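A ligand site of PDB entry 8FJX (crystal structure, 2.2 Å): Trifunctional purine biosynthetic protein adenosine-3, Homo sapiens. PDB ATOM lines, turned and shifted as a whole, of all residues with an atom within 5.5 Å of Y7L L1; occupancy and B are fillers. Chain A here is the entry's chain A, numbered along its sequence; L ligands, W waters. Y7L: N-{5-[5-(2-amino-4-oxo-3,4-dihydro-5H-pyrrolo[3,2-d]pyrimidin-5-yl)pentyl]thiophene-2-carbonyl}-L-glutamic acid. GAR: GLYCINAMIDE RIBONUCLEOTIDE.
The backbone carbonyl oxygen (O) of Glu 142 is in hydrogen-bond range of a nitrogen (N11) of Y7L L1 (3.1 Å). O of Leu 93 sits at hydrogen-bond distance from N11 of Y7L L1 (2.9 Å). The backbone carbonyl oxygen (O) of Met 90 is in hydrogen-bond range of a nitrogen (N19) of Y7L L1 (2.7 Å). An oxygen (O27) of Y7L L1 is in salt-bridge range of the guanidinium group (NH2) of Arg 65 (2.8 Å). The side-chain sulfur (SD) of Met 90 sits at hydrogen-bond distance from a nitrogen (N24) of GAR L2. O of Ala 141 is in hydrogen-bond range of N3 of Y7L L1 (2.9 Å). NH2 of Arg 91 is in salt-bridge range of O28 of Y7L L1 (3.5 Å). N of Ile 92 sits at hydrogen-bond distance from O28 of Y7L L1, 2.9 Å away. N of Leu 93 lies within hydrogen-bond range of N1 of Y7L L1 (2.9 Å).
The backbone carbonyl oxygen of Ile 92 lies within hydrogen-bond range of the guanidinium group of Arg 65, 2.9 Å away. The backbone NH (N) of Asn 107 lies within hydrogen-bond range of the backbone carbonyl oxygen (O) of His 138.
Leu 86 touches Y7L L1 (CD1 to C6, 3.6 Å). Val 98 touches Y7L L1 (CG2 to N11, 3.5 Å). Asn 107 touches Y7L L1. ND1 of His 109 touches C32 of Y7L L1 (3.5 Å). Gly 118 touches Y7L L1 (C to C33, 3.6 Å). CB of Ser 119 touches S12 of Y7L L1, 3.8 Å away. Val 140 touches Y7L L1 (CG1 to C4, 3.4 Å). Val 144 touches Y7L L1 (CG2 to C31, 3.6 Å). Hydrophobic or aromatic side chains that line Y7L L1: Leu 86, Met 90, Ile 92, Leu 93, Val 98, His 109, Val 140 and Val 144.
Water W1 lies within hydrogen-bond range of O10 of Y7L L1 (2.8 Å), N of Ala 141 (2.9 Å) and O of Asp 143 (3.1 Å).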
ATOM      1  N   ARG A  65      -3.956 -19.849 -10.135  1.00  0.00           N
ATOM      2  CA  ARG A  65      -5.069 -19.313 -10.897  1.00  0.00           C
ATOM      3  C   ARG A  65      -5.600 -18.023 -10.278  1.00  0.00           C
ATOM      4  O   ARG A  65      -5.989 -17.097 -10.997  1.00  0.00           O
ATOM      5  CB  ARG A  65      -6.185 -20.357 -11.014  1.00  0.00           C
ATOM      6  CG  ARG A  65      -5.682 -21.670 -11.587  1.00  0.00           C
ATOM      7  CD  ARG A  65      -6.807 -22.649 -11.890  1.00  0.00           C
ATOM      8  NE  ARG A  65      -6.281 -23.880 -12.472  1.00  0.00           N
ATOM      9  CZ  ARG A  65      -6.271 -24.156 -13.765  1.00  0.00           C
ATOM     10  NH1 ARG A  65      -6.756 -23.285 -14.646  1.00  0.00           N
ATOM     11  NH2 ARG A  65      -5.769 -25.306 -14.199  1.00  0.00           N
ATOM     12  N   LEU A  86     -16.647 -15.729 -22.469  1.00  0.00           N
ATOM     13  CA  LEU A  86     -15.512 -16.609 -22.772  1.00  0.00           C
ATOM     14  C   LEU A  86     -15.705 -17.135 -24.183  1.00  0.00           C
ATOM     15  O   LEU A  86     -16.666 -17.858 -24.459  1.00  0.00           O
ATOM     16  CB  LEU A  86     -15.440 -17.751 -21.758  1.00  0.00           C
ATOM     17  CG  LEU A  86     -15.451 -17.325 -20.283  1.00  0.00           C
ATOM     18  CD1 LEU A  86     -15.175 -18.507 -19.363  1.00  0.00           C
ATOM     19  CD2 LEU A  86     -14.458 -16.216 -20.041  1.00  0.00           C
ATOM     20  N   PHE A  89     -11.726 -19.285 -24.683  1.00  0.00           N
ATOM     21  CA  PHE A  89     -10.823 -19.142 -23.545  1.00  0.00           C
ATOM     22  C   PHE A  89     -10.501 -20.514 -22.979  1.00  0.00           C
ATOM     23  O   PHE A  89     -11.409 -21.260 -22.591  1.00  0.00           O
ATOM     24  CB  PHE A  89     -11.466 -18.251 -22.486  1.00  0.00           C
ATOM     25  CG  PHE A  89     -10.516 -17.763 -21.445  1.00  0.00           C
ATOM     26  CD1 PHE A  89      -9.490 -16.895 -21.799  1.00  0.00           C
ATOM     27  CD2 PHE A  89     -10.638 -18.166 -20.134  1.00  0.00           C
ATOM     28  CE1 PHE A  89      -8.605 -16.437 -20.851  1.00  0.00           C
ATOM     29  CE2 PHE A  89      -9.755 -17.711 -19.169  1.00  0.00           C
ATOM     30  CZ  PHE A  89      -8.737 -16.842 -19.530  1.00  0.00           C
ATOM     31  N   MET A  90      -9.208 -20.829 -22.901  1.00  0.00           N
ATOM     32  CA  MET A  90      -8.762 -22.176 -22.564  1.00  0.00           C
ATOM     33  C   MET A  90      -8.225 -22.305 -21.137  1.00  0.00           C
ATOM     34  O   MET A  90      -7.545 -23.282 -20.822  1.00  0.00           O
ATOM     35  CB  MET A  90      -7.689 -22.637 -23.564  1.00  0.00           C
ATOM     36  CG  MET A  90      -8.201 -22.873 -24.977  1.00  0.00           C
ATOM     37  SD  MET A  90      -9.699 -23.892 -25.026  1.00  0.00           S
ATOM     38  CE  MET A  90      -9.246 -25.229 -23.915  1.00  0.00           C
ATOM     39  N   ARG A  91      -8.526 -21.336 -20.266  1.00  0.00           N
ATOM     40  CA  ARG A  91      -8.078 -21.390 -18.874  1.00  0.00           C
ATOM     41  C   ARG A  91      -9.266 -21.625 -17.958  1.00  0.00           C
ATOM     42  O   ARG A  91     -10.252 -20.880 -18.019  1.00  0.00           O
ATOM     43  CB  ARG A  91      -7.353 -20.104 -18.480  1.00  0.00           C
ATOM     44  CG  ARG A  91      -6.121 -19.781 -19.309  1.00  0.00           C
ATOM     45  CD  ARG A  91      -5.131 -20.924 -19.269  1.00  0.00           C
ATOM     46  NE  ARG A  91      -4.892 -21.383 -17.898  1.00  0.00           N
ATOM     47  CZ  ARG A  91      -4.071 -22.376 -17.576  1.00  0.00           C
ATOM     48  NH1 ARG A  91      -3.401 -23.011 -18.530  1.00  0.00           N
ATOM     49  NH2 ARG A  91      -3.905 -22.716 -16.303  1.00  0.00           N
ATOM     50  N   ILE A  92      -9.176 -22.646 -17.114  1.00  0.00           N
ATOM     51  CA  ILE A  92     -10.162 -22.819 -16.064  1.00  0.00           C
ATOM     52  C   ILE A  92      -9.990 -21.705 -15.048  1.00  0.00           C
ATOM     53  O   ILE A  92      -8.865 -21.342 -14.672  1.00  0.00           O
ATOM     54  CB  ILE A  92     -10.022 -24.205 -15.414  1.00  0.00           C
ATOM     55  CG1 ILE A  92     -10.387 -25.296 -16.423  1.00  0.00           C
ATOM     56  CG2 ILE A  92     -10.911 -24.318 -14.187  1.00  0.00           C
ATOM     57  CD1 ILE A  92     -11.849 -25.249 -16.870  1.00  0.00           C
ATOM     58  N   LEU A  93     -11.107 -21.140 -14.602  1.00  0.00           N
ATOM     59  CA  LEU A  93     -11.106 -20.002 -13.695  1.00  0.00           C
ATOM     60  C   LEU A  93     -11.279 -20.468 -12.251  1.00  0.00           C
ATOM     61  O   LEU A  93     -11.873 -21.525 -11.993  1.00  0.00           O
ATOM     62  CB  LEU A  93     -12.208 -19.016 -14.076  1.00  0.00           C
ATOM     63  CG  LEU A  93     -12.118 -18.494 -15.516  1.00  0.00           C
ATOM     64  CD1 LEU A  93     -13.438 -17.867 -15.955  1.00  0.00           C
ATOM     65  CD2 LEU A  93     -10.973 -17.498 -15.642  1.00  0.00           C
ATOM     66  N   SER A  94     -10.759 -19.673 -11.327  1.00  0.00           N
ATOM     67  CA  SER A  94     -10.815 -20.025  -9.910  1.00  0.00           C
ATOM     68  C   SER A  94     -12.213 -19.803  -9.344  1.00  0.00           C
ATOM     69  O   SER A  94     -12.984 -18.973  -9.828  1.00  0.00           O
ATOM     70  CB  SER A  94      -9.803 -19.207  -9.118  1.00  0.00           C
ATOM     71  OG  SER A  94     -10.131 -17.826  -9.151  1.00  0.00           O
ATOM     72  N   GLY A  95     -12.522 -20.552  -8.290  1.00  0.00           N
ATOM     73  CA  GLY A  95     -13.817 -20.507  -7.660  1.00  0.00           C
ATOM     74  C   GLY A  95     -14.282 -19.116  -7.297  1.00  0.00           C
ATOM     75  O   GLY A  95     -15.384 -18.685  -7.650  1.00  0.00           O
ATOM     76  N   VAL A  98     -15.176 -17.122 -10.348  1.00  0.00           N
ATOM     77  CA  VAL A  98     -16.456 -17.566 -10.897  1.00  0.00           C
ATOM     78  C   VAL A  98     -17.597 -17.145  -9.986  1.00  0.00           C
ATOM     79  O   VAL A  98     -18.685 -16.762 -10.461  1.00  0.00           O
ATOM     80  CB  VAL A  98     -16.439 -19.086 -11.102  1.00  0.00           C
ATOM     81  CG1 VAL A  98     -17.799 -19.565 -11.606  1.00  0.00           C
ATOM     82  CG2 VAL A  98     -15.338 -19.483 -12.073  1.00  0.00           C
ATOM     83  N   ASN A 107     -20.254 -18.524 -21.640  1.00  0.00           N
ATOM     84  CA  ASN A 107     -19.262 -19.331 -22.324  1.00  0.00           C
ATOM     85  C   ASN A 107     -19.933 -20.086 -23.469  1.00  0.00           C
ATOM     86  O   ASN A 107     -21.072 -20.547 -23.332  1.00  0.00           O
ATOM     87  CB  ASN A 107     -18.593 -20.319 -21.379  1.00  0.00           C
ATOM     88  CG  ASN A 107     -17.696 -21.282 -22.093  1.00  0.00           C
ATOM     89  OD1 ASN A 107     -16.622 -20.896 -22.562  1.00  0.00           O
ATOM     90  ND2 ASN A 107     -18.133 -22.527 -22.223  1.00  0.00           N
ATOM     91  N   HIS A 109     -19.648 -23.428 -25.776  1.00  0.00           N
ATOM     92  CA  HIS A 109     -19.053 -24.749 -25.713  1.00  0.00           C
ATOM     93  C   HIS A 109     -19.518 -25.555 -26.925  1.00  0.00           C
ATOM     94  O   HIS A 109     -20.723 -25.577 -27.225  1.00  0.00           O
ATOM     95  CB  HIS A 109     -19.455 -25.472 -24.420  1.00  0.00           C
ATOM     96  CG  HIS A 109     -18.745 -26.768 -24.231  1.00  0.00           C
ATOM     97  ND1 HIS A 109     -17.434 -26.842 -23.810  1.00  0.00           N
ATOM     98  CD2 HIS A 109     -19.157 -28.048 -24.404  1.00  0.00           C
ATOM     99  CE1 HIS A 109     -17.068 -28.117 -23.730  1.00  0.00           C
ATOM    100  NE2 HIS A 109     -18.097 -28.859 -24.080  1.00  0.00           N
ATOM    101  N   LYS A 117     -18.417 -32.741 -22.078  1.00  0.00           N
ATOM    102  CA  LYS A 117     -17.803 -31.631 -21.379  1.00  0.00           C
ATOM    103  C   LYS A 117     -16.295 -31.645 -21.602  1.00  0.00           C
ATOM    104  O   LYS A 117     -15.719 -32.596 -22.149  1.00  0.00           O
ATOM    105  CB  LYS A 117     -18.124 -31.703 -19.889  1.00  0.00           C
ATOM    106  CG  LYS A 117     -19.557 -32.094 -19.616  1.00  0.00           C
ATOM    107  CD  LYS A 117     -20.043 -31.610 -18.253  1.00  0.00           C
ATOM    108  CE  LYS A 117     -21.427 -32.164 -17.961  1.00  0.00           C
ATOM    109  NZ  LYS A 117     -21.420 -33.649 -17.976  1.00  0.00           N
ATOM    110  N   GLY A 118     -15.633 -30.576 -21.184  1.00  0.00           N
ATOM    111  CA  GLY A 118     -14.196 -30.548 -21.281  1.00  0.00           C
ATOM    112  C   GLY A 118     -13.682 -30.128 -22.642  1.00  0.00           C
ATOM    113  O   GLY A 118     -14.411 -29.703 -23.536  1.00  0.00           O
ATOM    114  N   SER A 119     -12.366 -30.298 -22.800  1.00  0.00           N
ATOM    115  CA  SER A 119     -11.620 -29.507 -23.772  1.00  0.00           C
ATOM    116  C   SER A 119     -11.695 -30.049 -25.196  1.00  0.00           C
ATOM    117  O   SER A 119     -11.496 -29.273 -26.140  1.00  0.00           O
ATOM    118  CB  SER A 119     -10.162 -29.397 -23.335  1.00  0.00           C
ATOM    119  OG  SER A 119      -9.660 -30.670 -22.972  1.00  0.00           O
ATOM    120  N   HIS A 138     -23.794 -21.083 -22.090  1.00  0.00           N
ATOM    121  CA  HIS A 138     -24.245 -21.246 -20.725  1.00  0.00           C
ATOM    122  C   HIS A 138     -23.568 -20.232 -19.827  1.00  0.00           C
ATOM    123  O   HIS A 138     -22.496 -19.700 -20.143  1.00  0.00           O
ATOM    124  CB  HIS A 138     -23.958 -22.666 -20.210  1.00  0.00           C
ATOM    125  CG  HIS A 138     -22.501 -23.021 -20.196  1.00  0.00           C
ATOM    126  ND1 HIS A 138     -21.722 -22.911 -19.069  1.00  0.00           N
ATOM    127  CD2 HIS A 138     -21.687 -23.482 -21.175  1.00  0.00           C
ATOM    128  CE1 HIS A 138     -20.490 -23.290 -19.345  1.00  0.00           C
ATOM    129  NE2 HIS A 138     -20.439 -23.628 -20.624  1.00  0.00           N
ATOM    130  N   VAL A 140     -21.373 -19.531 -16.602  1.00  0.00           N
ATOM    131  CA  VAL A 140     -20.256 -20.260 -16.010  1.00  0.00           C
ATOM    132  C   VAL A 140     -20.492 -20.418 -14.510  1.00  0.00           C
ATOM    133  O   VAL A 140     -20.760 -19.441 -13.799  1.00  0.00           O
ATOM    134  CB  VAL A 140     -18.930 -19.543 -16.282  1.00  0.00           C
ATOM    135  CG1 VAL A 140     -17.781 -20.280 -15.605  1.00  0.00           C
ATOM    136  CG2 VAL A 140     -18.687 -19.436 -17.776  1.00  0.00           C
ATOM    137  N   ALA A 141     -20.427 -21.663 -14.031  1.00  0.00           N
ATOM    138  CA  ALA A 141     -20.379 -21.990 -12.611  1.00  0.00           C
ATOM    139  C   ALA A 141     -19.026 -22.607 -12.284  1.00  0.00           C
ATOM    140  O   ALA A 141     -18.168 -22.761 -13.161  1.00  0.00           O
ATOM    141  CB  ALA A 141     -21.534 -22.917 -12.232  1.00  0.00           C
ATOM    142  N   GLU A 142     -18.825 -22.958 -11.020  1.00  0.00           N
ATOM    143  CA  GLU A 142     -17.512 -23.466 -10.619  1.00  0.00           C
ATOM    144  C   GLU A 142     -17.099 -24.707 -11.391  1.00  0.00           C
ATOM    145  O   GLU A 142     -15.900 -24.979 -11.521  1.00  0.00           O
ATOM    146  CB  GLU A 142     -17.500 -23.728  -9.112  1.00  0.00           C
ATOM    147  CG  GLU A 142     -17.985 -22.552  -8.275  1.00  0.00           C
ATOM    148  CD  GLU A 142     -17.286 -22.424  -6.938  1.00  0.00           C
ATOM    149  OE1 GLU A 142     -16.464 -23.311  -6.602  1.00  0.00           O
ATOM    150  OE2 GLU A 142     -17.530 -21.431  -6.222  1.00  0.00           O
ATOM    151  N   ASP A 143     -18.064 -25.465 -11.918  1.00  0.00           N
ATOM    152  CA  ASP A 143     -17.801 -26.603 -12.791  1.00  0.00           C
ATOM    153  C   ASP A 143     -18.790 -26.580 -13.952  1.00  0.00           C
ATOM    154  O   ASP A 143     -19.891 -26.048 -13.824  1.00  0.00           O
ATOM    155  CB  ASP A 143     -17.910 -27.942 -12.026  1.00  0.00           C
ATOM    156  CG  ASP A 143     -19.169 -28.018 -11.180  1.00  0.00           C
ATOM    157  OD1 ASP A 143     -19.859 -26.982 -11.032  1.00  0.00           O
ATOM    158  OD2 ASP A 143     -19.467 -29.118 -10.668  1.00  0.00           O
ATOM    159  N   VAL A 144     -18.368 -27.147 -15.092  1.00  0.00           N
ATOM    160  CA  VAL A 144     -19.206 -27.106 -16.287  1.00  0.00           C
ATOM    161  C   VAL A 144     -20.567 -27.734 -16.067  1.00  0.00           C
ATOM    162  O   VAL A 144     -21.480 -27.565 -16.890  1.00  0.00           O
ATOM    163  CB  VAL A 144     -18.483 -27.786 -17.481  1.00  0.00           C
ATOM    164  CG1 VAL A 144     -19.307 -27.640 -18.766  1.00  0.00           C
ATOM    165  CG2 VAL A 144     -17.088 -27.216 -17.664  1.00  0.00           C
HETATM  166  C8  Y7L L   1     -15.180 -22.651 -16.993  1.00  0.00           C
HETATM  167  N7  Y7L L   1     -15.258 -22.515 -18.336  1.00  0.00           N
HETATM  168  C5  Y7L L   1     -13.342 -21.614 -17.720  1.00  0.00           C
HETATM  169  C6  Y7L L   1     -14.178 -21.894 -18.798  1.00  0.00           C
HETATM  170  N1  Y7L L   1     -13.760 -22.152 -15.217  1.00  0.00           N
HETATM  171  C2  Y7L L   1     -14.619 -22.710 -14.372  1.00  0.00           C
HETATM  172  N3  Y7L L   1     -15.768 -23.245 -14.767  1.00  0.00           N
HETATM  173  C4  Y7L L   1     -16.078 -23.233 -16.045  1.00  0.00           C
HETATM  174  C13 Y7L L   1     -10.259 -26.316 -20.111  1.00  0.00           C
HETATM  175  C14 Y7L L   1     -10.819 -25.062 -20.425  1.00  0.00           C
HETATM  176  C15 Y7L L   1     -12.204 -25.128 -20.808  1.00  0.00           C
HETATM  177  C16 Y7L L   1     -12.740 -26.422 -20.796  1.00  0.00           C
HETATM  178  C17 Y7L L   1      -8.851 -26.665 -19.650  1.00  0.00           C
HETATM  179  C20 Y7L L   1      -6.510 -26.077 -19.047  1.00  0.00           C
HETATM  180  C21 Y7L L   1      -5.483 -25.787 -20.142  1.00  0.00           C
HETATM  181  C22 Y7L L   1      -5.576 -26.872 -21.216  1.00  0.00           C
HETATM  182  C23 Y7L L   1      -4.741 -26.589 -22.473  1.00  0.00           C
HETATM  183  C26 Y7L L   1      -6.179 -25.367 -17.744  1.00  0.00           C
HETATM  184  C29 Y7L L   1     -16.378 -22.978 -19.140  1.00  0.00           C
HETATM  185  C30 Y7L L   1     -15.863 -23.627 -20.416  1.00  0.00           C
HETATM  186  C31 Y7L L   1     -15.770 -25.150 -20.285  1.00  0.00           C
HETATM  187  C32 Y7L L   1     -15.080 -25.736 -21.517  1.00  0.00           C
HETATM  188  C33 Y7L L   1     -14.161 -26.883 -21.140  1.00  0.00           C
HETATM  189  C9  Y7L L   1     -14.004 -22.105 -16.553  1.00  0.00           C
HETATM  190  N11 Y7L L   1     -14.284 -22.721 -12.957  1.00  0.00           N
HETATM  191  N19 Y7L L   1      -7.828 -25.650 -19.488  1.00  0.00           N
HETATM  192  O10 Y7L L   1     -17.289 -23.790 -16.490  1.00  0.00           O
HETATM  193  O18 Y7L L   1      -8.594 -27.790 -19.416  1.00  0.00           O
HETATM  194  O24 Y7L L   1      -3.761 -27.511 -22.856  1.00  0.00           O
HETATM  195  O25 Y7L L   1      -4.968 -25.437 -23.221  1.00  0.00           O
HETATM  196  O27 Y7L L   1      -5.342 -25.870 -16.942  1.00  0.00           O
HETATM  197  O28 Y7L L   1      -6.768 -24.285 -17.468  1.00  0.00           O
HETATM  198  S12 Y7L L   1     -11.490 -27.448 -20.310  1.00  0.00           S
HETATM  199  C1  GAR L   2     -14.939 -22.570 -30.536  1.00  0.00           C
HETATM  200  O6  GAR L   2     -15.177 -23.557 -31.536  1.00  0.00           O
HETATM  201  C2  GAR L   2     -15.578 -23.013 -29.214  1.00  0.00           C
HETATM  202  O8  GAR L   2     -16.714 -23.823 -29.444  1.00  0.00           O
HETATM  203  C3  GAR L   2     -14.417 -23.775 -28.552  1.00  0.00           C
HETATM  204  O4  GAR L   2     -13.216 -23.109 -28.983  1.00  0.00           O
HETATM  205  C5  GAR L   2     -13.430 -22.500 -30.262  1.00  0.00           C
HETATM  206  C10 GAR L   2     -12.940 -21.073 -30.296  1.00  0.00           C
HETATM  207  O12 GAR L   2     -12.842 -20.660 -31.655  1.00  0.00           O
HETATM  208  N19 GAR L   2     -14.557 -23.799 -27.130  1.00  0.00           N
HETATM  209  C21 GAR L   2     -13.808 -24.618 -26.395  1.00  0.00           C
HETATM  210  O22 GAR L   2     -13.057 -25.453 -26.868  1.00  0.00           O
HETATM  211  C23 GAR L   2     -13.968 -24.445 -24.903  1.00  0.00           C
HETATM  212  N24 GAR L   2     -12.794 -24.904 -24.195  1.00  0.00           N
HETATM  213  P15 GAR L   2     -12.675 -19.101 -31.988  1.00  0.00           P
HETATM  214  O16 GAR L   2     -13.931 -18.456 -31.429  1.00  0.00           O
HETATM  215  O17 GAR L   2     -11.395 -18.737 -31.244  1.00  0.00           O
HETATM  216  O18 GAR L   2     -12.592 -19.072 -33.497  1.00  0.00           O
HETATM  217  O   HOH W   1     -19.992 -23.778 -15.931  1.00  0.00           O
